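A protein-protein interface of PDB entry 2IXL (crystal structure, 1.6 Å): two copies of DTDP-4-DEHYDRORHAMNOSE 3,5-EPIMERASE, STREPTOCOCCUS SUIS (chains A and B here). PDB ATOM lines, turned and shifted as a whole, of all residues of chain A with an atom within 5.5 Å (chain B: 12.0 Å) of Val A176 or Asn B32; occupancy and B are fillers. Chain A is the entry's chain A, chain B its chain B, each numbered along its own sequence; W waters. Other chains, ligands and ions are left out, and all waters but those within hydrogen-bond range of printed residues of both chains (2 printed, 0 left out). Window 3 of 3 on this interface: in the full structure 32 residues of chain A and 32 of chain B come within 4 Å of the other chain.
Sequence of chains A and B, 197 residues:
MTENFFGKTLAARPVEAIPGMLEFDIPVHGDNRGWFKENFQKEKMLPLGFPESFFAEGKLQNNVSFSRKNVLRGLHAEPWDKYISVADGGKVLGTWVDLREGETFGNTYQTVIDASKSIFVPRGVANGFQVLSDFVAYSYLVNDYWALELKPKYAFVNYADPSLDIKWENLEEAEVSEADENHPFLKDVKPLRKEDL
Among the printed residues, merely in contact across the chains: Arg A68 with Gly B34, Val A71 with Arg B33, Val A176 with Asn B32 and Ser A177 with Arg B33.
Printed residues of chain B within 4 Å of Arg A68: Asn B32 (2.7 Å), Arg B33 (3.3 Å) and Gly B34 (3.97 Å).
Val A71 touches one residue of chain B.
No residue of chain B comes within 4 Å of Leu A72.
Printed residues of chain B within 4 Å of Glu A175: Asn B32 (2.8 Å).
Glu A178 touches none of the printed residues of chain B.
No residue of chain B comes within 4 Å of Asp A180.
Phe B6 touches none of the printed residues of chain A.
Of chain A, only Arg A68 (2.7 Å), Glu A175 (2.8 Å) and Val A176 (3.5 Å) come within 4 Å of Asn B32.
Printed residues of chain A within 4 Å of Arg B33: Arg A68, Val A71 and Ser A177.
Of the printed residues of chain A, Gly B34 touches Arg A68 (3.97 Å).
The nearest residue of chain B that does not touch Val A176 is Arg B33 (4.2 Å).
The nearest residue of chain A that does not touch Asn B32 is Ser A177 (5.0 Å).
O of Glu A175 is in hydrogen-bond range of N of Leu A72, at 3.0 Å.
The side-chain hydroxyl of Ser A177 lies within hydrogen-bond range of the backbone NH of Asp A180, 2.9 Å away.
OD2 of Asp B31 lies within salt-bridge range of NH2 of Arg B33, 3.0 Å away.
The side-chain carboxylate of Asp B31 lies within hydrogen-bond range of the backbone NH of Gly B34.
Of the 11 printed residues of chain A, 5 touch a printed residue of chain B.
Hydrophobic or aromatic side chains of chain A that line the printed part of chain B: Val A71.
Printed residues of chain B that touch a printed residue of chain A: Asn B32, Arg B33 and Gly B34.
Along chain B the printed residues that touch a printed residue of chain A span positions 32 to 34.
Among the printed residues, no Asp or Glu carboxylate lies within 4 Å of a Lys or Arg side-chain nitrogen of the other chain.
No position is printed for both chains.
Water W1 lies within hydrogen-bond range of the guanidinium group (NH1) of Arg A68, the backbone NH (N) of Gly B34 and the backbone carbonyl oxygen (O) of Arg B33.
Water W2 lies within hydrogen-bond range of O of Leu A72 (2.7 Å), OD2 of Asp A180 (2.7 Å), N of Ser A177 (2.9 Å) and NH1 of Arg B33 (3.0 Å).
The backbone carbonyl oxygen (O) of Asn B32 sits at hydrogen-bond distance from the guanidinium group (NH1) of Arg A68 (2.7 Å).
The backbone carbonyl oxygen (O) of Arg B33 lies within hydrogen-bond range of the backbone NH (N) of Arg A68, 3.3 Å away.
ND2 of Asn B32 is in hydrogen-bond range of OE2 of Glu A175.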
ATOM      1  N   ARG A  68     -10.658  -3.151  -7.197  1.00  0.00           N
ATOM      2  CA  ARG A  68      -9.630  -4.181  -7.434  1.00  0.00           C
ATOM      3  C   ARG A  68      -9.539  -5.209  -6.306  1.00  0.00           C
ATOM      4  O   ARG A  68     -10.041  -4.983  -5.207  1.00  0.00           O
ATOM      5  CB  ARG A  68      -8.257  -3.532  -7.595  1.00  0.00           C
ATOM      6  CG  ARG A  68      -8.151  -2.489  -8.687  1.00  0.00           C
ATOM      7  CD  ARG A  68      -6.713  -2.013  -8.818  1.00  0.00           C
ATOM      8  NE  ARG A  68      -6.066  -1.891  -7.510  1.00  0.00           N
ATOM      9  CZ  ARG A  68      -6.227  -0.861  -6.681  1.00  0.00           C
ATOM     10  NH1 ARG A  68      -7.007   0.158  -7.017  1.00  0.00           N
ATOM     11  NH2 ARG A  68      -5.609  -0.853  -5.511  1.00  0.00           N
ATOM     12  N   VAL A  71      -9.492  -4.900  -2.078  1.00  0.00           N
ATOM     13  CA  VAL A  71     -10.265  -3.731  -1.639  1.00  0.00           C
ATOM     14  C   VAL A  71     -11.377  -4.189  -0.677  1.00  0.00           C
ATOM     15  O   VAL A  71     -12.068  -5.182  -0.929  1.00  0.00           O
ATOM     16  CB  VAL A  71     -10.874  -2.951  -2.843  1.00  0.00           C
ATOM     17  CG1 VAL A  71     -11.977  -1.971  -2.393  1.00  0.00           C
ATOM     18  CG2 VAL A  71      -9.783  -2.210  -3.619  1.00  0.00           C
ATOM     19  N   LEU A  72     -11.511  -3.471   0.440  1.00  0.00           N
ATOM     20  CA  LEU A  72     -12.551  -3.736   1.437  1.00  0.00           C
ATOM     21  C   LEU A  72     -13.296  -2.415   1.691  1.00  0.00           C
ATOM     22  O   LEU A  72     -12.658  -1.407   2.005  1.00  0.00           O
ATOM     23  CB  LEU A  72     -11.896  -4.294   2.721  1.00  0.00           C
ATOM     24  CG  LEU A  72     -12.741  -4.889   3.855  1.00  0.00           C
ATOM     25  CD1 LEU A  72     -11.842  -5.673   4.821  1.00  0.00           C
ATOM     26  CD2 LEU A  72     -13.537  -3.820   4.626  1.00  0.00           C
ATOM     27  N   TYR A 159     -14.423  -1.846  10.249  1.00  0.00           N
ATOM     28  CA  TYR A 159     -14.226  -3.183   9.660  1.00  0.00           C
ATOM     29  C   TYR A 159     -13.307  -4.095  10.480  1.00  0.00           C
ATOM     30  O   TYR A 159     -13.452  -5.324  10.441  1.00  0.00           O
ATOM     31  CB  TYR A 159     -13.690  -3.063   8.223  1.00  0.00           C
ATOM     32  CG  TYR A 159     -12.215  -2.743   8.133  1.00  0.00           C
ATOM     33  CD1 TYR A 159     -11.272  -3.756   7.916  1.00  0.00           C
ATOM     34  CD2 TYR A 159     -11.759  -1.440   8.275  1.00  0.00           C
ATOM     35  CE1 TYR A 159      -9.919  -3.468   7.837  1.00  0.00           C
ATOM     36  CE2 TYR A 159     -10.408  -1.141   8.200  1.00  0.00           C
ATOM     37  CZ  TYR A 159      -9.494  -2.161   7.985  1.00  0.00           C
ATOM     38  OH  TYR A 159      -8.146  -1.865   7.915  1.00  0.00           O
ATOM     39  N   ALA A 174      -5.919  -5.871   3.267  1.00  0.00           N
ATOM     40  CA  ALA A 174      -7.083  -5.054   2.907  1.00  0.00           C
ATOM     41  C   ALA A 174      -6.700  -3.648   2.437  1.00  0.00           C
ATOM     42  O   ALA A 174      -5.860  -2.977   3.057  1.00  0.00           O
ATOM     43  CB  ALA A 174      -8.095  -4.989   4.075  1.00  0.00           C
ATOM     44  N   GLU A 175      -7.299  -3.222   1.327  1.00  0.00           N
ATOM     45  CA  GLU A 175      -7.091  -1.877   0.794  1.00  0.00           C
ATOM     46  C   GLU A 175      -8.350  -1.043   1.057  1.00  0.00           C
ATOM     47  O   GLU A 175      -9.412  -1.282   0.474  1.00  0.00           O
ATOM     48  CB  GLU A 175      -6.751  -1.917  -0.700  1.00  0.00           C
ATOM     49  CG  GLU A 175      -6.539  -0.543  -1.352  1.00  0.00           C
ATOM     50  CD  GLU A 175      -5.153   0.069  -1.082  1.00  0.00           C
ATOM     51  OE1 GLU A 175      -4.219  -0.646  -0.634  1.00  0.00           O
ATOM     52  OE2 GLU A 175      -4.992   1.287  -1.329  1.00  0.00           O
ATOM     53  N   VAL A 176      -8.210  -0.053   1.934  1.00  0.00           N
ATOM     54  CA  VAL A 176      -9.357   0.665   2.493  1.00  0.00           C
ATOM     55  C   VAL A 176      -9.241   2.196   2.312  1.00  0.00           C
ATOM     56  O   VAL A 176      -8.147   2.727   2.079  1.00  0.00           O
ATOM     57  CB  VAL A 176      -9.540   0.276   4.006  1.00  0.00           C
ATOM     58  CG1 VAL A 176     -10.758   0.892   4.588  1.00  0.00           C
ATOM     59  CG2 VAL A 176      -9.638  -1.240   4.180  1.00  0.00           C
ATOM     60  N   SER A 177     -10.371   2.896   2.407  1.00  0.00           N
ATOM     61  CA  SER A 177     -10.382   4.365   2.408  1.00  0.00           C
ATOM     62  C   SER A 177      -9.898   4.931   3.741  1.00  0.00           C
ATOM     63  O   SER A 177      -9.943   4.250   4.778  1.00  0.00           O
ATOM     64  CB  SER A 177     -11.796   4.887   2.123  1.00  0.00           C
ATOM     65  OG  SER A 177     -12.690   4.556   3.187  1.00  0.00           O
ATOM     66  N   GLU A 178      -9.456   6.194   3.716  1.00  0.00           N
ATOM     67  CA  GLU A 178      -9.159   6.935   4.951  1.00  0.00           C
ATOM     68  C   GLU A 178     -10.355   6.954   5.910  1.00  0.00           C
ATOM     69  O   GLU A 178     -10.187   6.769   7.110  1.00  0.00           O
ATOM     70  CB  GLU A 178      -8.701   8.363   4.643  1.00  0.00           C
ATOM     71  CG  GLU A 178      -7.239   8.458   4.245  1.00  0.00           C
ATOM     72  CD  GLU A 178      -6.586   9.778   4.633  1.00  0.00           C
ATOM     73  OE1 GLU A 178      -7.076  10.467   5.561  1.00  0.00           O
ATOM     74  OE2 GLU A 178      -5.556  10.122   4.009  1.00  0.00           O
ATOM     75  N   ASP A 180     -12.844   4.691   6.120  1.00  0.00           N
ATOM     76  CA  ASP A 180     -13.077   3.362   6.687  1.00  0.00           C
ATOM     77  C   ASP A 180     -12.054   2.972   7.747  1.00  0.00           C
ATOM     78  O   ASP A 180     -12.328   2.133   8.612  1.00  0.00           O
ATOM     79  CB  ASP A 180     -13.189   2.303   5.582  1.00  0.00           C
ATOM     80  CG  ASP A 180     -14.544   2.322   4.900  1.00  0.00           C
ATOM     81  OD1 ASP A 180     -15.454   2.975   5.449  1.00  0.00           O
ATOM     82  OD2 ASP A 180     -14.716   1.673   3.835  1.00  0.00           O
ATOM     83  N   GLU A 181     -10.877   3.586   7.688  1.00  0.00           N
ATOM     84  CA  GLU A 181      -9.875   3.397   8.731  1.00  0.00           C
ATOM     85  C   GLU A 181     -10.310   4.007  10.068  1.00  0.00           C
ATOM     86  O   GLU A 181      -9.926   3.513  11.129  1.00  0.00           O
ATOM     87  CB  GLU A 181      -8.527   3.979   8.291  1.00  0.00           C
ATOM     88  CG  GLU A 181      -7.822   3.140   7.229  1.00  0.00           C
ATOM     89  CD  GLU A 181      -6.435   3.652   6.869  1.00  0.00           C
ATOM     90  OE1 GLU A 181      -5.965   4.632   7.487  1.00  0.00           O
ATOM     91  OE2 GLU A 181      -5.804   3.059   5.965  1.00  0.00           O
ATOM     92  N   PHE B   6     -13.103  10.924 -15.662  1.00  0.00           N
ATOM     93  CA  PHE B   6     -13.413  11.306 -14.275  1.00  0.00           C
ATOM     94  C   PHE B   6     -13.899  12.744 -14.162  1.00  0.00           C
ATOM     95  O   PHE B   6     -13.518  13.591 -14.969  1.00  0.00           O
ATOM     96  CB  PHE B   6     -12.185  11.135 -13.380  1.00  0.00           C
ATOM     97  CG  PHE B   6     -11.722   9.716 -13.242  1.00  0.00           C
ATOM     98  CD1 PHE B   6     -10.518   9.299 -13.806  1.00  0.00           C
ATOM     99  CD2 PHE B   6     -12.488   8.786 -12.543  1.00  0.00           C
ATOM    100  CE1 PHE B   6     -10.081   7.972 -13.665  1.00  0.00           C
ATOM    101  CE2 PHE B   6     -12.066   7.464 -12.400  1.00  0.00           C
ATOM    102  CZ  PHE B   6     -10.855   7.055 -12.959  1.00  0.00           C
ATOM    103  N   VAL B  28     -17.990  10.566 -12.318  1.00  0.00           N
ATOM    104  CA  VAL B  28     -17.328   9.348 -11.855  1.00  0.00           C
ATOM    105  C   VAL B  28     -16.139   9.781 -11.004  1.00  0.00           C
ATOM    106  O   VAL B  28     -15.299  10.561 -11.454  1.00  0.00           O
ATOM    107  CB  VAL B  28     -16.878   8.433 -13.030  1.00  0.00           C
ATOM    108  CG1 VAL B  28     -16.297   7.107 -12.493  1.00  0.00           C
ATOM    109  CG2 VAL B  28     -18.043   8.159 -13.984  1.00  0.00           C
ATOM    110  N   HIS B  29     -16.112   9.296  -9.765  1.00  0.00           N
ATOM    111  CA  HIS B  29     -15.135   9.715  -8.760  1.00  0.00           C
ATOM    112  C   HIS B  29     -14.122   8.603  -8.538  1.00  0.00           C
ATOM    113  O   HIS B  29     -14.492   7.525  -8.086  1.00  0.00           O
ATOM    114  CB  HIS B  29     -15.868  10.035  -7.452  1.00  0.00           C
ATOM    115  CG  HIS B  29     -16.934  11.077  -7.606  1.00  0.00           C
ATOM    116  ND1 HIS B  29     -18.281  10.789  -7.532  1.00  0.00           N
ATOM    117  CD2 HIS B  29     -16.846  12.402  -7.871  1.00  0.00           C
ATOM    118  CE1 HIS B  29     -18.975  11.899  -7.717  1.00  0.00           C
ATOM    119  NE2 HIS B  29     -18.128  12.891  -7.926  1.00  0.00           N
ATOM    120  N   GLY B  30     -12.853   8.867  -8.869  1.00  0.00           N
ATOM    121  CA  GLY B  30     -11.785   7.871  -8.739  1.00  0.00           C
ATOM    122  C   GLY B  30     -10.894   8.051  -7.516  1.00  0.00           C
ATOM    123  O   GLY B  30     -10.681   9.175  -7.060  1.00  0.00           O
ATOM    124  N   ASP B  31     -10.390   6.931  -6.985  1.00  0.00           N
ATOM    125  CA  ASP B  31      -9.437   6.915  -5.848  1.00  0.00           C
ATOM    126  C   ASP B  31      -8.558   5.655  -5.863  1.00  0.00           C
ATOM    127  O   ASP B  31      -8.478   4.970  -6.888  1.00  0.00           O
ATOM    128  CB  ASP B  31     -10.153   7.092  -4.493  1.00  0.00           C
ATOM    129  CG  ASP B  31     -10.928   5.853  -4.051  1.00  0.00           C
ATOM    130  OD1 ASP B  31     -10.869   4.806  -4.726  1.00  0.00           O
ATOM    131  OD2 ASP B  31     -11.604   5.937  -3.004  1.00  0.00           O
ATOM    132  N   ASN B  32      -7.915   5.352  -4.725  1.00  0.00           N
ATOM    133  CA  ASN B  32      -6.972   4.231  -4.611  1.00  0.00           C
ATOM    134  C   ASN B  32      -7.612   2.840  -4.727  1.00  0.00           C
ATOM    135  O   ASN B  32      -6.916   1.835  -4.921  1.00  0.00           O
ATOM    136  CB  ASN B  32      -6.197   4.317  -3.283  1.00  0.00           C
ATOM    137  CG  ASN B  32      -7.122   4.280  -2.065  1.00  0.00           C
ATOM    138  OD1 ASN B  32      -8.030   5.101  -1.936  1.00  0.00           O
ATOM    139  ND2 ASN B  32      -6.894   3.323  -1.173  1.00  0.00           N
ATOM    140  N   ARG B  33      -8.931   2.792  -4.600  1.00  0.00           N
ATOM    141  CA  ARG B  33      -9.664   1.525  -4.605  1.00  0.00           C
ATOM    142  C   ARG B  33     -10.213   1.168  -5.994  1.00  0.00           C
ATOM    143  O   ARG B  33     -10.456  -0.008  -6.288  1.00  0.00           O
ATOM    144  CB  ARG B  33     -10.808   1.569  -3.584  1.00  0.00           C
ATOM    145  CG  ARG B  33     -10.373   1.624  -2.110  1.00  0.00           C
ATOM    146  CD  ARG B  33     -11.554   1.949  -1.194  1.00  0.00           C
ATOM    147  NE  ARG B  33     -12.243   3.183  -1.586  1.00  0.00           N
ATOM    148  CZ  ARG B  33     -13.382   3.627  -1.058  1.00  0.00           C
ATOM    149  NH1 ARG B  33     -13.990   2.951  -0.087  1.00  0.00           N
ATOM    150  NH2 ARG B  33     -13.921   4.758  -1.509  1.00  0.00           N
ATOM    151  N   GLY B  34     -10.417   2.191  -6.823  1.00  0.00           N
ATOM    152  CA  GLY B  34     -11.170   2.085  -8.081  1.00  0.00           C
ATOM    153  C   GLY B  34     -11.988   3.347  -8.300  1.00  0.00           C
ATOM    154  O   GLY B  34     -11.446   4.452  -8.253  1.00  0.00           O
ATOM    155  N   TRP B  35     -13.297   3.201  -8.506  1.00  0.00           N
ATOM    156  CA  TRP B  35     -14.178   4.357  -8.676  1.00  0.00           C
ATOM    157  C   TRP B  35     -15.622   4.110  -8.214  1.00  0.00           C
ATOM    158  O   TRP B  35     -16.016   2.978  -7.923  1.00  0.00           O
ATOM    159  CB  TRP B  35     -14.131   4.938 -10.113  1.00  0.00           C
ATOM    160  CG  TRP B  35     -14.369   3.981 -11.305  1.00  0.00           C
ATOM    161  CD1 TRP B  35     -13.420   3.512 -12.172  1.00  0.00           C
ATOM    162  CD2 TRP B  35     -15.620   3.443 -11.763  1.00  0.00           C
ATOM    163  NE1 TRP B  35     -13.990   2.709 -13.134  1.00  0.00           N
ATOM    164  CE2 TRP B  35     -15.339   2.645 -12.915  1.00  0.00           C
ATOM    165  CE3 TRP B  35     -16.944   3.537 -11.313  1.00  0.00           C
ATOM    166  CZ2 TRP B  35     -16.348   1.952 -13.625  1.00  0.00           C
ATOM    167  CZ3 TRP B  35     -17.949   2.844 -12.016  1.00  0.00           C
ATOM    168  CH2 TRP B  35     -17.638   2.063 -13.162  1.00  0.00           C
ATOM    169  N   PHE B  36     -16.383   5.201  -8.145  1.00  0.00           N
ATOM    170  CA  PHE B  36     -17.786   5.205  -7.698  1.00  0.00           C
ATOM    171  C   PHE B  36     -18.589   6.193  -8.560  1.00  0.00           C
ATOM    172  O   PHE B  36     -18.095   7.279  -8.856  1.00  0.00           O
ATOM    173  CB  PHE B  36     -17.864   5.649  -6.227  1.00  0.00           C
ATOM    174  CG  PHE B  36     -19.253   5.577  -5.647  1.00  0.00           C
ATOM    175  CD1 PHE B  36     -19.608   4.516  -4.828  1.00  0.00           C
ATOM    176  CD2 PHE B  36     -20.205   6.570  -5.924  1.00  0.00           C
ATOM    177  CE1 PHE B  36     -20.899   4.422  -4.292  1.00  0.00           C
ATOM    178  CE2 PHE B  36     -21.516   6.480  -5.402  1.00  0.00           C
ATOM    179  CZ  PHE B  36     -21.846   5.398  -4.585  1.00  0.00           C
HETATM  180  O   HOH W   1      -8.596   0.587  -9.140  1.00  0.00           O
HETATM  181  O   HOH W   2     -12.732   1.286   2.001  1.00  0.00           O
